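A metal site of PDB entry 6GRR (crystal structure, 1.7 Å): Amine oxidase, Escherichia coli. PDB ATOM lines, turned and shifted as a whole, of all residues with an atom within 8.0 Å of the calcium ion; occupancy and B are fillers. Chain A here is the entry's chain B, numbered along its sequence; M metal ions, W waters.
OD2 of Asp 528 lies within salt-bridge range of NZ of Lys 128, at 2.6 Å.
N of Tyr 353 lies within hydrogen-bond range of O of Asp 528, at 2.8 Å.
N of Asp 528 sits at hydrogen-bond distance from O of Glu 354 (2.8 Å).
The side-chain amino group of Lys 128 is in salt-bridge range of the side-chain carboxylate of Asp 530 (3.2 Å).
The backbone NH (N) of Asp 530 is in hydrogen-bond range of the backbone carbonyl oxygen (O) of Val 351, 2.9 Å away.
The side-chain carboxylate (OD2) of Asp 530 lies within hydrogen-bond range of the indole nitrogen (NE1) of Trp 132 (2.9 Å).
OD2 of Asp 673 is in salt-bridge range of NZ of Lys 128 (2.7 Å).
The backbone carbonyl oxygen (O) of Asp 673 is in hydrogen-bond range of the backbone NH (N) of Tyr 638 (2.8 Å).
Merely in contact with the calcium ion: Lys 128 (3.8 Å).
Within 4 Å of the calcium ion: Lys 128, Asp 528, Leu 529, Asp 530, Asp 673 and Ala 674.
The calcium ion is bound by OD1 of Asp 528, O of Ala 674, OD1 of Asp 530, OD1 of Asp 673, O of Leu 529 and water W1.
Water W1 lies within hydrogen-bond range of the backbone carbonyl oxygen of Glu 534 (2.7 Å), the side-chain amide oxygen of Asn 536 (2.8 Å) and the backbone NH of Ala 674 (3.0 Å).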
ATOM      1  N   LYS A 128      -2.060  24.837  23.240  1.00  0.00           N
ATOM      2  CA  LYS A 128      -1.926  25.949  22.287  1.00  0.00           C
ATOM      3  C   LYS A 128      -3.252  26.481  21.767  1.00  0.00           C
ATOM      4  O   LYS A 128      -3.464  27.679  21.729  1.00  0.00           O
ATOM      5  CB  LYS A 128      -1.027  25.562  21.085  1.00  0.00           C
ATOM      6  CG  LYS A 128      -1.030  26.520  19.894  1.00  0.00           C
ATOM      7  CD  LYS A 128       0.041  26.098  18.899  1.00  0.00           C
ATOM      8  CE  LYS A 128       0.184  27.060  17.740  1.00  0.00           C
ATOM      9  NZ  LYS A 128       1.436  26.784  17.013  1.00  0.00           N
ATOM     10  N   TRP A 132      -4.586  30.383  22.306  1.00  0.00           N
ATOM     11  CA  TRP A 132      -5.016  31.275  21.229  1.00  0.00           C
ATOM     12  C   TRP A 132      -6.467  31.709  21.409  1.00  0.00           C
ATOM     13  O   TRP A 132      -6.799  32.852  21.147  1.00  0.00           O
ATOM     14  CB  TRP A 132      -4.893  30.644  19.846  1.00  0.00           C
ATOM     15  CG  TRP A 132      -3.613  30.900  19.084  1.00  0.00           C
ATOM     16  CD1 TRP A 132      -2.859  29.974  18.432  1.00  0.00           C
ATOM     17  CD2 TRP A 132      -2.973  32.172  18.847  1.00  0.00           C
ATOM     18  NE1 TRP A 132      -1.802  30.583  17.800  1.00  0.00           N
ATOM     19  CE2 TRP A 132      -1.834  31.924  18.052  1.00  0.00           C
ATOM     20  CE3 TRP A 132      -3.246  33.488  19.250  1.00  0.00           C
ATOM     21  CZ2 TRP A 132      -0.972  32.946  17.631  1.00  0.00           C
ATOM     22  CZ3 TRP A 132      -2.364  34.511  18.842  1.00  0.00           C
ATOM     23  CH2 TRP A 132      -1.266  34.232  18.030  1.00  0.00           C
ATOM     24  N   VAL A 351       0.245  36.115  14.006  1.00  0.00           N
ATOM     25  CA  VAL A 351       1.581  36.134  13.369  1.00  0.00           C
ATOM     26  C   VAL A 351       2.461  35.041  14.007  1.00  0.00           C
ATOM     27  O   VAL A 351       3.066  34.248  13.269  1.00  0.00           O
ATOM     28  CB  VAL A 351       2.251  37.519  13.472  1.00  0.00           C
ATOM     29  CG1 VAL A 351       3.654  37.498  12.848  1.00  0.00           C
ATOM     30  CG2 VAL A 351       1.405  38.556  12.773  1.00  0.00           C
ATOM     31  N   MET A 352       2.568  35.015  15.335  1.00  0.00           N
ATOM     32  CA  MET A 352       3.476  34.080  16.012  1.00  0.00           C
ATOM     33  C   MET A 352       2.941  33.617  17.336  1.00  0.00           C
ATOM     34  O   MET A 352       2.622  34.425  18.188  1.00  0.00           O
ATOM     35  CB  MET A 352       4.864  34.727  16.193  1.00  0.00           C
ATOM     36  CG  MET A 352       5.893  33.809  16.873  1.00  0.00           C
ATOM     37  SD  MET A 352       7.582  34.429  16.706  1.00  0.00           S
ATOM     38  CE  MET A 352       7.539  35.847  17.790  1.00  0.00           C
ATOM     39  N   TYR A 353       2.820  32.292  17.510  1.00  0.00           N
ATOM     40  CA  TYR A 353       2.367  31.750  18.787  1.00  0.00           C
ATOM     41  C   TYR A 353       3.417  31.877  19.894  1.00  0.00           C
ATOM     42  O   TYR A 353       3.103  32.331  20.996  1.00  0.00           O
ATOM     43  CB  TYR A 353       1.862  30.289  18.659  1.00  0.00           C
ATOM     44  CG  TYR A 353       1.424  29.756  20.009  1.00  0.00           C
ATOM     45  CD1 TYR A 353       0.313  30.308  20.660  1.00  0.00           C
ATOM     46  CD2 TYR A 353       2.142  28.762  20.665  1.00  0.00           C
ATOM     47  CE1 TYR A 353      -0.050  29.877  21.915  1.00  0.00           C
ATOM     48  CE2 TYR A 353       1.773  28.285  21.923  1.00  0.00           C
ATOM     49  CZ  TYR A 353       0.670  28.849  22.540  1.00  0.00           C
ATOM     50  OH  TYR A 353       0.291  28.405  23.775  1.00  0.00           O
ATOM     51  N   GLU A 354       4.645  31.488  19.612  1.00  0.00           N
ATOM     52  CA  GLU A 354       5.744  31.616  20.557  1.00  0.00           C
ATOM     53  C   GLU A 354       7.021  31.797  19.744  1.00  0.00           C
ATOM     54  O   GLU A 354       7.263  31.072  18.791  1.00  0.00           O
ATOM     55  CB  GLU A 354       5.942  30.378  21.443  1.00  0.00           C
ATOM     56  CG  GLU A 354       4.838  30.069  22.450  1.00  0.00           C
ATOM     57  CD  GLU A 354       5.077  28.762  23.204  1.00  0.00           C
ATOM     58  OE1 GLU A 354       5.074  27.659  22.597  1.00  0.00           O
ATOM     59  OE2 GLU A 354       5.279  28.841  24.429  1.00  0.00           O
ATOM     60  N   ARG A 526      13.972  29.844  17.818  1.00  0.00           N
ATOM     61  CA  ARG A 526      12.790  29.040  17.570  1.00  0.00           C
ATOM     62  C   ARG A 526      11.579  29.921  17.445  1.00  0.00           C
ATOM     63  O   ARG A 526      11.183  30.573  18.398  1.00  0.00           O
ATOM     64  CB  ARG A 526      12.612  28.056  18.730  1.00  0.00           C
ATOM     65  CG  ARG A 526      11.377  27.175  18.594  1.00  0.00           C
ATOM     66  CD  ARG A 526      11.175  26.369  19.865  1.00  0.00           C
ATOM     67  NE  ARG A 526       9.987  25.537  19.699  1.00  0.00           N
ATOM     68  CZ  ARG A 526       8.723  25.961  19.805  1.00  0.00           C
ATOM     69  NH1 ARG A 526       8.444  27.211  20.153  1.00  0.00           N
ATOM     70  NH2 ARG A 526       7.731  25.127  19.575  1.00  0.00           N
ATOM     71  N   LEU A 527      10.945  29.888  16.277  1.00  0.00           N
ATOM     72  CA  LEU A 527       9.886  30.788  15.916  1.00  0.00           C
ATOM     73  C   LEU A 527       8.667  29.999  15.435  1.00  0.00           C
ATOM     74  O   LEU A 527       8.584  29.597  14.256  1.00  0.00           O
ATOM     75  CB  LEU A 527      10.358  31.711  14.809  1.00  0.00           C
ATOM     76  CG  LEU A 527      11.638  32.502  15.119  1.00  0.00           C
ATOM     77  CD1 LEU A 527      12.015  33.259  13.859  1.00  0.00           C
ATOM     78  CD2 LEU A 527      11.447  33.448  16.296  1.00  0.00           C
ATOM     79  N   ASP A 528       7.724  29.788  16.352  1.00  0.00           N
ATOM     80  CA  ASP A 528       6.469  29.148  15.978  1.00  0.00           C
ATOM     81  C   ASP A 528       5.545  30.180  15.395  1.00  0.00           C
ATOM     82  O   ASP A 528       4.584  30.635  16.046  1.00  0.00           O
ATOM     83  CB  ASP A 528       5.854  28.412  17.173  1.00  0.00           C
ATOM     84  CG  ASP A 528       4.519  27.725  16.833  1.00  0.00           C
ATOM     85  OD1 ASP A 528       4.153  27.560  15.642  1.00  0.00           O
ATOM     86  OD2 ASP A 528       3.823  27.403  17.802  1.00  0.00           O
ATOM     87  N   LEU A 529       5.838  30.566  14.143  1.00  0.00           N
ATOM     88  CA  LEU A 529       4.993  31.458  13.351  1.00  0.00           C
ATOM     89  C   LEU A 529       3.703  30.697  13.041  1.00  0.00           C
ATOM     90  O   LEU A 529       3.756  29.507  12.787  1.00  0.00           O
ATOM     91  CB  LEU A 529       5.679  31.853  12.040  1.00  0.00           C
ATOM     92  CG  LEU A 529       7.020  32.577  12.200  1.00  0.00           C
ATOM     93  CD1 LEU A 529       7.725  32.764  10.883  1.00  0.00           C
ATOM     94  CD2 LEU A 529       6.803  33.906  12.893  1.00  0.00           C
ATOM     95  N   ASP A 530       2.572  31.378  13.151  1.00  0.00           N
ATOM     96  CA  ASP A 530       1.266  30.897  12.708  1.00  0.00           C
ATOM     97  C   ASP A 530       0.757  31.994  11.808  1.00  0.00           C
ATOM     98  O   ASP A 530       0.109  32.944  12.279  1.00  0.00           O
ATOM     99  CB  ASP A 530       0.295  30.730  13.893  1.00  0.00           C
ATOM    100  CG  ASP A 530       0.575  29.506  14.744  1.00  0.00           C
ATOM    101  OD1 ASP A 530       1.396  28.648  14.398  1.00  0.00           O
ATOM    102  OD2 ASP A 530      -0.048  29.418  15.830  1.00  0.00           O
ATOM    103  N   VAL A 531       1.072  31.896  10.521  1.00  0.00           N
ATOM    104  CA  VAL A 531       0.847  32.974   9.587  1.00  0.00           C
ATOM    105  C   VAL A 531      -0.636  33.079   9.230  1.00  0.00           C
ATOM    106  O   VAL A 531      -1.115  32.377   8.348  1.00  0.00           O
ATOM    107  CB  VAL A 531       1.723  32.840   8.334  1.00  0.00           C
ATOM    108  CG1 VAL A 531       1.426  33.925   7.301  1.00  0.00           C
ATOM    109  CG2 VAL A 531       3.192  32.888   8.757  1.00  0.00           C
ATOM    110  N   GLY A 533      -3.000  32.038  10.929  1.00  0.00           N
ATOM    111  CA  GLY A 533      -3.555  30.708  11.144  1.00  0.00           C
ATOM    112  C   GLY A 533      -2.480  29.678  11.411  1.00  0.00           C
ATOM    113  O   GLY A 533      -1.294  29.900  11.132  1.00  0.00           O
ATOM    114  N   GLU A 534      -2.937  28.546  11.929  1.00  0.00           N
ATOM    115  CA  GLU A 534      -2.128  27.361  12.256  1.00  0.00           C
ATOM    116  C   GLU A 534      -1.530  26.715  11.015  1.00  0.00           C
ATOM    117  O   GLU A 534      -0.350  26.373  10.966  1.00  0.00           O
ATOM    118  CB  GLU A 534      -3.057  26.342  12.962  1.00  0.00           C
ATOM    119  CG  GLU A 534      -2.440  25.046  13.464  1.00  0.00           C
ATOM    120  CD  GLU A 534      -3.475  24.025  13.954  1.00  0.00           C
ATOM    121  OE1 GLU A 534      -4.676  24.381  14.123  1.00  0.00           O
ATOM    122  OE2 GLU A 534      -3.093  22.862  14.177  1.00  0.00           O
ATOM    123  N   ASN A 535      -2.368  26.516  10.005  1.00  0.00           N
ATOM    124  CA  ASN A 535      -1.996  25.650   8.883  1.00  0.00           C
ATOM    125  C   ASN A 535      -1.263  26.428   7.788  1.00  0.00           C
ATOM    126  O   ASN A 535      -1.830  27.271   7.097  1.00  0.00           O
ATOM    127  CB  ASN A 535      -3.243  24.914   8.360  1.00  0.00           C
ATOM    128  CG  ASN A 535      -3.814  23.977   9.425  1.00  0.00           C
ATOM    129  OD1 ASN A 535      -3.083  23.248  10.095  1.00  0.00           O
ATOM    130  ND2 ASN A 535      -5.119  24.023   9.601  1.00  0.00           N
ATOM    131  N   ASN A 536       0.031  26.135   7.677  1.00  0.00           N
ATOM    132  CA  ASN A 536       0.970  26.837   6.828  1.00  0.00           C
ATOM    133  C   ASN A 536       1.807  25.848   5.986  1.00  0.00           C
ATOM    134  O   ASN A 536       1.883  24.640   6.303  1.00  0.00           O
ATOM    135  CB  ASN A 536       1.951  27.653   7.688  1.00  0.00           C
ATOM    136  CG  ASN A 536       1.284  28.768   8.506  1.00  0.00           C
ATOM    137  OD1 ASN A 536       1.906  29.293   9.444  1.00  0.00           O
ATOM    138  ND2 ASN A 536       0.062  29.160   8.152  1.00  0.00           N
ATOM    139  N   LEU A 583       6.959  31.355   4.692  1.00  0.00           N
ATOM    140  CA  LEU A 583       5.966  30.525   5.361  1.00  0.00           C
ATOM    141  C   LEU A 583       4.618  31.101   4.983  1.00  0.00           C
ATOM    142  O   LEU A 583       4.283  32.232   5.360  1.00  0.00           O
ATOM    143  CB  LEU A 583       6.185  30.490   6.868  1.00  0.00           C
ATOM    144  CG  LEU A 583       5.349  29.471   7.641  1.00  0.00           C
ATOM    145  CD1 LEU A 583       5.702  28.045   7.232  1.00  0.00           C
ATOM    146  CD2 LEU A 583       5.467  29.634   9.144  1.00  0.00           C
ATOM    147  N   THR A 636       9.983  22.446  11.229  1.00  0.00           N
ATOM    148  CA  THR A 636       9.473  21.210  11.814  1.00  0.00           C
ATOM    149  C   THR A 636       8.016  21.338  12.142  1.00  0.00           C
ATOM    150  O   THR A 636       7.442  22.418  12.107  1.00  0.00           O
ATOM    151  CB  THR A 636      10.210  20.842  13.103  1.00  0.00           C
ATOM    152  OG1 THR A 636      10.091  21.917  14.050  1.00  0.00           O
ATOM    153  CG2 THR A 636      11.649  20.610  12.815  1.00  0.00           C
ATOM    154  N   ARG A 637       7.396  20.211  12.453  1.00  0.00           N
ATOM    155  CA  ARG A 637       5.999  20.218  12.850  1.00  0.00           C
ATOM    156  C   ARG A 637       5.903  20.608  14.312  1.00  0.00           C
ATOM    157  O   ARG A 637       6.753  20.187  15.137  1.00  0.00           O
ATOM    158  CB  ARG A 637       5.362  18.847  12.599  1.00  0.00           C
ATOM    159  CG  ARG A 637       5.260  18.478  11.132  1.00  0.00           C
ATOM    160  CD  ARG A 637       4.865  17.014  10.958  1.00  0.00           C
ATOM    161  NE  ARG A 637       3.505  16.777  11.448  1.00  0.00           N
ATOM    162  CZ  ARG A 637       2.381  16.904  10.736  1.00  0.00           C
ATOM    163  NH1 ARG A 637       2.400  17.232   9.450  1.00  0.00           N
ATOM    164  NH2 ARG A 637       1.219  16.667  11.320  1.00  0.00           N
ATOM    165  N   TYR A 638       4.905  21.425  14.643  1.00  0.00           N
ATOM    166  CA  TYR A 638       4.688  21.870  16.028  1.00  0.00           C
ATOM    167  C   TYR A 638       4.601  20.684  16.980  1.00  0.00           C
ATOM    168  O   TYR A 638       3.799  19.782  16.790  1.00  0.00           O
ATOM    169  CB  TYR A 638       3.419  22.731  16.176  1.00  0.00           C
ATOM    170  CG  TYR A 638       3.085  23.015  17.624  1.00  0.00           C
ATOM    171  CD1 TYR A 638       3.835  23.934  18.363  1.00  0.00           C
ATOM    172  CD2 TYR A 638       2.021  22.364  18.268  1.00  0.00           C
ATOM    173  CE1 TYR A 638       3.548  24.186  19.712  1.00  0.00           C
ATOM    174  CE2 TYR A 638       1.736  22.614  19.608  1.00  0.00           C
ATOM    175  CZ  TYR A 638       2.490  23.523  20.318  1.00  0.00           C
ATOM    176  OH  TYR A 638       2.205  23.776  21.636  1.00  0.00           O
ATOM    177  N   THR A 672       0.086  22.547   7.477  1.00  0.00           N
ATOM    178  CA  THR A 672       0.094  22.069   8.847  1.00  0.00           C
ATOM    179  C   THR A 672       0.784  23.073   9.782  1.00  0.00           C
ATOM    180  O   THR A 672       1.376  24.055   9.311  1.00  0.00           O
ATOM    181  CB  THR A 672       0.772  20.685   8.930  1.00  0.00           C
ATOM    182  OG1 THR A 672       0.491  20.075  10.201  1.00  0.00           O
ATOM    183  CG2 THR A 672       2.282  20.783   8.751  1.00  0.00           C
ATOM    184  N   ASP A 673       0.746  22.798  11.081  1.00  0.00           N
ATOM    185  CA  ASP A 673       1.362  23.673  12.067  1.00  0.00           C
ATOM    186  C   ASP A 673       2.892  23.570  12.049  1.00  0.00           C
ATOM    187  O   ASP A 673       3.473  22.572  12.484  1.00  0.00           O
ATOM    188  CB  ASP A 673       0.800  23.430  13.465  1.00  0.00           C
ATOM    189  CG  ASP A 673       1.137  24.563  14.433  1.00  0.00           C
ATOM    190  OD1 ASP A 673       1.892  25.465  14.023  1.00  0.00           O
ATOM    191  OD2 ASP A 673       0.682  24.561  15.603  1.00  0.00           O
ATOM    192  N   ALA A 674       3.539  24.614  11.546  1.00  0.00           N
ATOM    193  CA  ALA A 674       4.983  24.629  11.351  1.00  0.00           C
ATOM    194  C   ALA A 674       5.684  25.464  12.394  1.00  0.00           C
ATOM    195  O   ALA A 674       5.122  26.438  12.913  1.00  0.00           O
ATOM    196  CB  ALA A 674       5.311  25.147   9.968  1.00  0.00           C
ATOM    197  N   VAL A 675       6.914  25.087  12.691  1.00  0.00           N
ATOM    198  CA  VAL A 675       7.795  25.852  13.562  1.00  0.00           C
ATOM    199  C   VAL A 675       9.067  26.111  12.755  1.00  0.00           C
ATOM    200  O   VAL A 675       9.637  25.180  12.193  1.00  0.00           O
ATOM    201  CB  VAL A 675       8.140  25.114  14.864  1.00  0.00           C
ATOM    202  CG1 VAL A 675       9.132  25.903  15.702  1.00  0.00           C
ATOM    203  CG2 VAL A 675       6.880  24.850  15.706  1.00  0.00           C
ATOM    204  N   VAL A 676       9.468  27.376  12.685  1.00  0.00           N
ATOM    205  CA  VAL A 676      10.660  27.796  11.932  1.00  0.00           C
ATOM    206  C   VAL A 676      11.815  27.974  12.902  1.00  0.00           C
ATOM    207  O   VAL A 676      11.652  28.550  13.956  1.00  0.00           O
ATOM    208  CB  VAL A 676      10.372  29.122  11.185  1.00  0.00           C
ATOM    209  CG1 VAL A 676      11.651  29.728  10.588  1.00  0.00           C
ATOM    210  CG2 VAL A 676       9.328  28.884  10.103  1.00  0.00           C
HETATM  211 CA    CA M   1       3.178  27.394  13.658  1.00  0.00          CA
HETATM  212  O   HOH W   1       2.128  27.290  11.452  1.00  0.00           O
